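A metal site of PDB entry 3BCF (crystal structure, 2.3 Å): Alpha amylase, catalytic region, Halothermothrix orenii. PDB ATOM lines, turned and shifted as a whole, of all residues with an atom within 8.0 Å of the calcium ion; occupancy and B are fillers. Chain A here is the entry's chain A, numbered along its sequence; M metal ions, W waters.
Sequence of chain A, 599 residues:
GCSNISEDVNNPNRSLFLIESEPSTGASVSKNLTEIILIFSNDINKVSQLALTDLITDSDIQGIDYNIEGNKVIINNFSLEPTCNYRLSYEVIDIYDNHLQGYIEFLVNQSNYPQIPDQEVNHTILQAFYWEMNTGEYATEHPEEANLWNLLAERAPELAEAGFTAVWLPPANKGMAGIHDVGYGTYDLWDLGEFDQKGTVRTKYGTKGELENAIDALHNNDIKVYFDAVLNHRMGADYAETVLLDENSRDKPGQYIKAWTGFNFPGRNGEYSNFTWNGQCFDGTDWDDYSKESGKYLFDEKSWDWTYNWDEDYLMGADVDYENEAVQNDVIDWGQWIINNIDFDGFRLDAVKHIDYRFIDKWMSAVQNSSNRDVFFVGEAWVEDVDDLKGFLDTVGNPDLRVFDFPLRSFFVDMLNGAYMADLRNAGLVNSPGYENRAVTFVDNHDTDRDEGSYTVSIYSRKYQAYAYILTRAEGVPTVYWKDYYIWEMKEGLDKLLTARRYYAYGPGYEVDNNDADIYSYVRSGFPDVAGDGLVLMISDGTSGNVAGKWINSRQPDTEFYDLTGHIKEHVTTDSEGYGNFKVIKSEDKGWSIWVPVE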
ATOM      1  N   LEU A 231       7.472 -12.560  -4.905  1.00  0.00           N
ATOM      2  CA  LEU A 231       8.298 -12.612  -6.116  1.00  0.00           C
ATOM      3  C   LEU A 231       8.802 -11.291  -6.579  1.00  0.00           C
ATOM      4  O   LEU A 231       9.408 -11.235  -7.651  1.00  0.00           O
ATOM      5  CB  LEU A 231       7.389 -13.082  -7.315  1.00  0.00           C
ATOM      6  CG  LEU A 231       6.887 -14.494  -7.198  1.00  0.00           C
ATOM      7  CD1 LEU A 231       6.123 -15.001  -8.480  1.00  0.00           C
ATOM      8  CD2 LEU A 231       7.999 -15.436  -6.735  1.00  0.00           C
ATOM      9  N   ASN A 232       8.397 -10.222  -5.922  1.00  0.00           N
ATOM     10  CA  ASN A 232       8.701  -8.845  -6.398  1.00  0.00           C
ATOM     11  C   ASN A 232      10.143  -8.412  -6.095  1.00  0.00           C
ATOM     12  O   ASN A 232      10.717  -7.655  -6.871  1.00  0.00           O
ATOM     13  CB  ASN A 232       7.735  -7.852  -5.692  1.00  0.00           C
ATOM     14  CG  ASN A 232       8.202  -6.388  -5.767  1.00  0.00           C
ATOM     15  OD1 ASN A 232       8.150  -5.746  -6.821  1.00  0.00           O
ATOM     16  ND2 ASN A 232       8.688  -5.878  -4.651  1.00  0.00           N
ATOM     17  N   HIS A 233      10.697  -8.813  -4.980  1.00  0.00           N
ATOM     18  CA  HIS A 233      11.984  -8.299  -4.527  1.00  0.00           C
ATOM     19  C   HIS A 233      12.886  -9.315  -3.773  1.00  0.00           C
ATOM     20  O   HIS A 233      12.470 -10.467  -3.470  1.00  0.00           O
ATOM     21  CB  HIS A 233      11.775  -7.145  -3.592  1.00  0.00           C
ATOM     22  CG  HIS A 233      10.970  -7.505  -2.404  1.00  0.00           C
ATOM     23  ND1 HIS A 233       9.695  -7.028  -2.217  1.00  0.00           N
ATOM     24  CD2 HIS A 233      11.229  -8.318  -1.344  1.00  0.00           C
ATOM     25  CE1 HIS A 233       9.203  -7.538  -1.098  1.00  0.00           C
ATOM     26  NE2 HIS A 233      10.110  -8.334  -0.556  1.00  0.00           N
ATOM     27  N   ASP A 283      16.343  -4.499 -11.331  1.00  0.00           N
ATOM     28  CA  ASP A 283      16.140  -3.251 -12.049  1.00  0.00           C
ATOM     29  C   ASP A 283      16.625  -2.175 -11.188  1.00  0.00           C
ATOM     30  O   ASP A 283      17.018  -1.171 -11.677  1.00  0.00           O
ATOM     31  CB  ASP A 283      14.674  -3.014 -12.368  1.00  0.00           C
ATOM     32  CG  ASP A 283      14.203  -3.759 -13.624  1.00  0.00           C
ATOM     33  OD1 ASP A 283      15.013  -3.875 -14.555  1.00  0.00           O
ATOM     34  OD2 ASP A 283      12.975  -4.209 -13.697  1.00  0.00           O
ATOM     35  N   TRP A 304      12.184  -0.189 -15.689  1.00  0.00           N
ATOM     36  CA  TRP A 304      11.179  -0.637 -14.810  1.00  0.00           C
ATOM     37  C   TRP A 304      10.197  -1.461 -15.681  1.00  0.00           C
ATOM     38  O   TRP A 304       9.935  -1.088 -16.843  1.00  0.00           O
ATOM     39  CB  TRP A 304      10.455   0.564 -14.234  1.00  0.00           C
ATOM     40  CG  TRP A 304      11.273   1.393 -13.254  1.00  0.00           C
ATOM     41  CD1 TRP A 304      11.386   2.729 -13.259  1.00  0.00           C
ATOM     42  CD2 TRP A 304      12.037   0.923 -12.152  1.00  0.00           C
ATOM     43  NE1 TRP A 304      12.199   3.133 -12.237  1.00  0.00           N
ATOM     44  CE2 TRP A 304      12.605   2.034 -11.542  1.00  0.00           C
ATOM     45  CE3 TRP A 304      12.303  -0.333 -11.613  1.00  0.00           C
ATOM     46  CZ2 TRP A 304      13.420   1.930 -10.444  1.00  0.00           C
ATOM     47  CZ3 TRP A 304      13.099  -0.440 -10.543  1.00  0.00           C
ATOM     48  CH2 TRP A 304      13.632   0.669  -9.936  1.00  0.00           C
ATOM     49  N   ASP A 305       9.768  -2.599 -15.145  1.00  0.00           N
ATOM     50  CA  ASP A 305       8.978  -3.537 -15.869  1.00  0.00           C
ATOM     51  C   ASP A 305       7.576  -3.033 -16.010  1.00  0.00           C
ATOM     52  O   ASP A 305       7.147  -2.206 -15.232  1.00  0.00           O
ATOM     53  CB  ASP A 305       8.940  -4.905 -15.159  1.00  0.00           C
ATOM     54  CG  ASP A 305      10.332  -5.501 -14.956  1.00  0.00           C
ATOM     55  OD1 ASP A 305      11.135  -5.354 -15.919  1.00  0.00           O
ATOM     56  OD2 ASP A 305      10.575  -6.101 -13.870  1.00  0.00           O
ATOM     57  N   THR A 307       3.797  -2.534 -15.651  1.00  0.00           N
ATOM     58  CA  THR A 307       2.907  -2.713 -14.523  1.00  0.00           C
ATOM     59  C   THR A 307       1.638  -1.961 -14.822  1.00  0.00           C
ATOM     60  O   THR A 307       1.690  -0.998 -15.565  1.00  0.00           O
ATOM     61  CB  THR A 307       3.521  -2.173 -13.147  1.00  0.00           C
ATOM     62  OG1 THR A 307       4.020  -0.841 -13.312  1.00  0.00           O
ATOM     63  CG2 THR A 307       4.651  -3.127 -12.593  1.00  0.00           C
ATOM     64  N   GLU A 312       5.065   1.661 -10.898  1.00  0.00           N
ATOM     65  CA  GLU A 312       4.859   0.919  -9.652  1.00  0.00           C
ATOM     66  C   GLU A 312       5.602  -0.435  -9.583  1.00  0.00           C
ATOM     67  O   GLU A 312       5.333  -1.250  -8.689  1.00  0.00           O
ATOM     68  CB  GLU A 312       3.354   0.676  -9.403  1.00  0.00           C
ATOM     69  CG  GLU A 312       2.557   1.921  -9.077  1.00  0.00           C
ATOM     70  CD  GLU A 312       1.223   1.592  -8.350  1.00  0.00           C
ATOM     71  OE1 GLU A 312       0.530   0.549  -8.680  1.00  0.00           O
ATOM     72  OE2 GLU A 312       0.920   2.394  -7.426  1.00  0.00           O
ATOM     73  N   ASP A 313       6.489  -0.693 -10.535  1.00  0.00           N
ATOM     74  CA  ASP A 313       7.419  -1.873 -10.460  1.00  0.00           C
ATOM     75  C   ASP A 313       8.209  -1.724  -9.141  1.00  0.00           C
ATOM     76  O   ASP A 313       8.210  -2.670  -8.319  1.00  0.00           O
ATOM     77  CB  ASP A 313       8.340  -1.941 -11.709  1.00  0.00           C
ATOM     78  CG  ASP A 313       9.211  -3.202 -11.729  1.00  0.00           C
ATOM     79  OD1 ASP A 313       8.957  -4.153 -10.953  1.00  0.00           O
ATOM     80  OD2 ASP A 313      10.198  -3.241 -12.533  1.00  0.00           O
ATOM     81  N   TYR A 314       8.769  -0.544  -8.890  1.00  0.00           N
ATOM     82  CA  TYR A 314       9.637  -0.377  -7.695  1.00  0.00           C
ATOM     83  C   TYR A 314       8.834  -0.226  -6.441  1.00  0.00           C
ATOM     84  O   TYR A 314       8.051   0.747  -6.309  1.00  0.00           O
ATOM     85  CB  TYR A 314      10.623   0.811  -7.743  1.00  0.00           C
ATOM     86  CG  TYR A 314      11.566   0.624  -6.568  1.00  0.00           C
ATOM     87  CD1 TYR A 314      12.497  -0.421  -6.583  1.00  0.00           C
ATOM     88  CD2 TYR A 314      11.396   1.325  -5.400  1.00  0.00           C
ATOM     89  CE1 TYR A 314      13.276  -0.741  -5.469  1.00  0.00           C
ATOM     90  CE2 TYR A 314      12.201   1.029  -4.262  1.00  0.00           C
ATOM     91  CZ  TYR A 314      13.142  -0.003  -4.317  1.00  0.00           C
ATOM     92  OH  TYR A 314      13.917  -0.344  -3.224  1.00  0.00           O
ATOM     93  N   LEU A 315       9.079  -1.115  -5.468  1.00  0.00           N
ATOM     94  CA  LEU A 315       8.387  -1.025  -4.161  1.00  0.00           C
ATOM     95  C   LEU A 315       9.326  -0.906  -2.953  1.00  0.00           C
ATOM     96  O   LEU A 315       9.210   0.003  -2.158  1.00  0.00           O
ATOM     97  CB  LEU A 315       7.465  -2.236  -3.936  1.00  0.00           C
ATOM     98  CG  LEU A 315       6.568  -2.242  -2.702  1.00  0.00           C
ATOM     99  CD1 LEU A 315       5.680  -0.978  -2.586  1.00  0.00           C
ATOM    100  CD2 LEU A 315       5.697  -3.521  -2.778  1.00  0.00           C
ATOM    101  N   MET A 316      10.194  -1.907  -2.805  1.00  0.00           N
ATOM    102  CA  MET A 316      11.117  -2.002  -1.649  1.00  0.00           C
ATOM    103  C   MET A 316      12.209  -3.013  -2.031  1.00  0.00           C
ATOM    104  O   MET A 316      12.016  -3.788  -2.996  1.00  0.00           O
ATOM    105  CB  MET A 316      10.348  -2.474  -0.419  1.00  0.00           C
ATOM    106  CG  MET A 316      10.034  -3.965  -0.427  1.00  0.00           C
ATOM    107  SD  MET A 316       8.961  -4.477   0.940  1.00  0.00           S
ATOM    108  CE  MET A 316       7.456  -4.753  -0.019  1.00  0.00           C
ATOM    109  N   ALA A 318      15.738  -4.957  -3.241  1.00  0.00           N
ATOM    110  CA  ALA A 318      16.317  -5.042  -4.534  1.00  0.00           C
ATOM    111  C   ALA A 318      15.153  -5.583  -5.525  1.00  0.00           C
ATOM    112  O   ALA A 318      14.683  -6.687  -5.373  1.00  0.00           O
ATOM    113  CB  ALA A 318      17.464  -6.048  -4.498  1.00  0.00           C
ATOM    114  N   ASP A 319      14.825  -4.822  -6.550  1.00  0.00           N
ATOM    115  CA  ASP A 319      13.729  -5.137  -7.423  1.00  0.00           C
ATOM    116  C   ASP A 319      14.054  -6.103  -8.571  1.00  0.00           C
ATOM    117  O   ASP A 319      14.866  -5.798  -9.462  1.00  0.00           O
ATOM    118  CB  ASP A 319      13.155  -3.857  -8.038  1.00  0.00           C
ATOM    119  CG  ASP A 319      11.764  -4.130  -8.721  1.00  0.00           C
ATOM    120  OD1 ASP A 319      10.800  -4.303  -7.895  1.00  0.00           O
ATOM    121  OD2 ASP A 319      11.685  -4.104 -10.010  1.00  0.00           O
ATOM    122  N   VAL A 320      13.391  -7.262  -8.570  1.00  0.00           N
ATOM    123  CA  VAL A 320      13.625  -8.268  -9.637  1.00  0.00           C
ATOM    124  C   VAL A 320      13.349  -7.705 -11.025  1.00  0.00           C
ATOM    125  O   VAL A 320      12.470  -6.869 -11.145  1.00  0.00           O
ATOM    126  CB  VAL A 320      12.859  -9.554  -9.343  1.00  0.00           C
ATOM    127  CG1 VAL A 320      13.158 -10.641 -10.372  1.00  0.00           C
ATOM    128  CG2 VAL A 320      13.288  -9.975  -7.921  1.00  0.00           C
ATOM    129  N   ASP A 321      14.215  -8.032 -12.003  1.00  0.00           N
ATOM    130  CA  ASP A 321      14.068  -7.591 -13.351  1.00  0.00           C
ATOM    131  C   ASP A 321      13.402  -8.718 -14.104  1.00  0.00           C
ATOM    132  O   ASP A 321      14.094  -9.632 -14.522  1.00  0.00           O
ATOM    133  CB  ASP A 321      15.401  -7.285 -14.011  1.00  0.00           C
ATOM    134  CG  ASP A 321      15.240  -6.865 -15.513  1.00  0.00           C
ATOM    135  OD1 ASP A 321      14.058  -6.759 -15.976  1.00  0.00           O
ATOM    136  OD2 ASP A 321      16.305  -6.618 -16.191  1.00  0.00           O
ATOM    137  N   TYR A 322      12.087  -8.725 -14.222  1.00  0.00           N
ATOM    138  CA  TYR A 322      11.423  -9.833 -14.914  1.00  0.00           C
ATOM    139  C   TYR A 322      11.506  -9.718 -16.414  1.00  0.00           C
ATOM    140  O   TYR A 322      10.994 -10.543 -17.124  1.00  0.00           O
ATOM    141  CB  TYR A 322       9.974 -10.067 -14.399  1.00  0.00           C
ATOM    142  CG  TYR A 322       9.981 -10.780 -13.056  1.00  0.00           C
ATOM    143  CD1 TYR A 322       9.685 -10.083 -11.868  1.00  0.00           C
ATOM    144  CD2 TYR A 322      10.436 -12.125 -12.956  1.00  0.00           C
ATOM    145  CE1 TYR A 322       9.757 -10.740 -10.594  1.00  0.00           C
ATOM    146  CE2 TYR A 322      10.537 -12.767 -11.678  1.00  0.00           C
ATOM    147  CZ  TYR A 322      10.164 -12.083 -10.535  1.00  0.00           C
ATOM    148  OH  TYR A 322      10.254 -12.736  -9.345  1.00  0.00           O
ATOM    149  N   ALA A 351       2.100  -8.689  -3.571  1.00  0.00           N
ATOM    150  CA  ALA A 351       2.461  -7.462  -4.332  1.00  0.00           C
ATOM    151  C   ALA A 351       2.318  -7.662  -5.762  1.00  0.00           C
ATOM    152  O   ALA A 351       3.142  -7.275  -6.529  1.00  0.00           O
ATOM    153  CB  ALA A 351       3.942  -6.875  -3.944  1.00  0.00           C
ATOM    154  N   VAL A 352       1.144  -8.196  -6.167  1.00  0.00           N
ATOM    155  CA  VAL A 352       0.989  -8.668  -7.493  1.00  0.00           C
ATOM    156  C   VAL A 352       0.982  -7.527  -8.483  1.00  0.00           C
ATOM    157  O   VAL A 352       1.447  -7.711  -9.630  1.00  0.00           O
ATOM    158  CB  VAL A 352      -0.247  -9.550  -7.606  1.00  0.00           C
ATOM    159  CG1 VAL A 352      -1.480  -8.748  -7.577  1.00  0.00           C
ATOM    160  CG2 VAL A 352      -0.114 -10.448  -8.767  1.00  0.00           C
ATOM    161  N   LYS A 353       0.510  -6.330  -8.110  1.00  0.00           N
ATOM    162  CA  LYS A 353       0.550  -5.254  -9.098  1.00  0.00           C
ATOM    163  C   LYS A 353       1.920  -4.533  -9.228  1.00  0.00           C
ATOM    164  O   LYS A 353       2.114  -3.791 -10.178  1.00  0.00           O
ATOM    165  CB  LYS A 353      -0.675  -4.305  -8.951  1.00  0.00           C
ATOM    166  CG  LYS A 353      -0.715  -3.366  -7.801  1.00  0.00           C
ATOM    167  CD  LYS A 353      -2.102  -2.571  -7.802  1.00  0.00           C
ATOM    168  CE  LYS A 353      -2.100  -1.345  -6.751  1.00  0.00           C
ATOM    169  NZ  LYS A 353      -1.152  -1.504  -5.543  1.00  0.00           N
ATOM    170  N   HIS A 354       2.879  -4.864  -8.374  1.00  0.00           N
ATOM    171  CA  HIS A 354       4.251  -4.346  -8.532  1.00  0.00           C
ATOM    172  C   HIS A 354       5.233  -5.286  -9.290  1.00  0.00           C
ATOM    173  O   HIS A 354       6.370  -5.111  -9.276  1.00  0.00           O
ATOM    174  CB  HIS A 354       4.810  -3.970  -7.194  1.00  0.00           C
ATOM    175  CG  HIS A 354       3.902  -3.075  -6.394  1.00  0.00           C
ATOM    176  ND1 HIS A 354       3.729  -1.730  -6.687  1.00  0.00           N
ATOM    177  CD2 HIS A 354       3.060  -3.345  -5.363  1.00  0.00           C
ATOM    178  CE1 HIS A 354       2.829  -1.214  -5.867  1.00  0.00           C
ATOM    179  NE2 HIS A 354       2.416  -2.158  -5.048  1.00  0.00           N
ATOM    180  N   ILE A 355       4.705  -6.202 -10.096  1.00  0.00           N
ATOM    181  CA  ILE A 355       5.530  -7.219 -10.730  1.00  0.00           C
ATOM    182  C   ILE A 355       5.002  -7.286 -12.144  1.00  0.00           C
ATOM    183  O   ILE A 355       3.803  -7.253 -12.323  1.00  0.00           O
ATOM    184  CB  ILE A 355       5.395  -8.671 -10.075  1.00  0.00           C
ATOM    185  CG1 ILE A 355       5.794  -8.601  -8.603  1.00  0.00           C
ATOM    186  CG2 ILE A 355       6.246  -9.756 -10.918  1.00  0.00           C
ATOM    187  CD1 ILE A 355       5.578  -9.841  -7.715  1.00  0.00           C
ATOM    188  N   ASP A 356       5.922  -7.385 -13.115  1.00  0.00           N
ATOM    189  CA  ASP A 356       5.648  -7.335 -14.482  1.00  0.00           C
ATOM    190  C   ASP A 356       4.345  -8.098 -14.874  1.00  0.00           C
ATOM    191  O   ASP A 356       4.242  -9.325 -14.828  1.00  0.00           O
ATOM    192  CB  ASP A 356       6.842  -7.924 -15.214  1.00  0.00           C
ATOM    193  CG  ASP A 356       6.765  -7.712 -16.714  1.00  0.00           C
ATOM    194  OD1 ASP A 356       5.669  -7.969 -17.377  1.00  0.00           O
ATOM    195  OD2 ASP A 356       7.859  -7.312 -17.217  1.00  0.00           O
HETATM  196 CA    CA M   1       8.697  -4.826  -8.810  1.00  0.00          CA
HETATM  197  O   HOH W   1       9.534  -6.980  -9.244  1.00  0.00           O
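The backbone carbonyl oxygen of Asn 232 is in hydrogen-bond range of the backbone NH of Val 320, 3.2 Å away. A ring nitrogen (ND1) of His 233 lies within hydrogen-bond range of the side-chain amide nitrogen (ND2) of Asn 232, 2.9 Å away. OD2 of Asp 313 lies within hydrogen-bond range of N of Asp 305, 2.7 Å away. N of Asp 283 sits at hydrogen-bond distance from O of Asp 319, at 2.7 Å. O of Glu 312 lies within hydrogen-bond range of ND1 of His 354, at 2.6 Å.
Water W1 bridges O of Asn 232 (2.7 Å) and O of Val 320 (3.5 Å).
The nearest printed residue that does not touch the calcium ion is Tyr 314 (4.3 Å).
The calcium ion is bound by OD1 of Asn 232 (2.3 Å), OD1 of Asp 313 (2.3 Å), O of Asp 313 (2.3 Å), water W1 (2.4 Å), OD1 of Asp 319 (2.4 Å) and O of His 354 (2.4 Å). The calcium ion has six donor atoms within binding distance.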
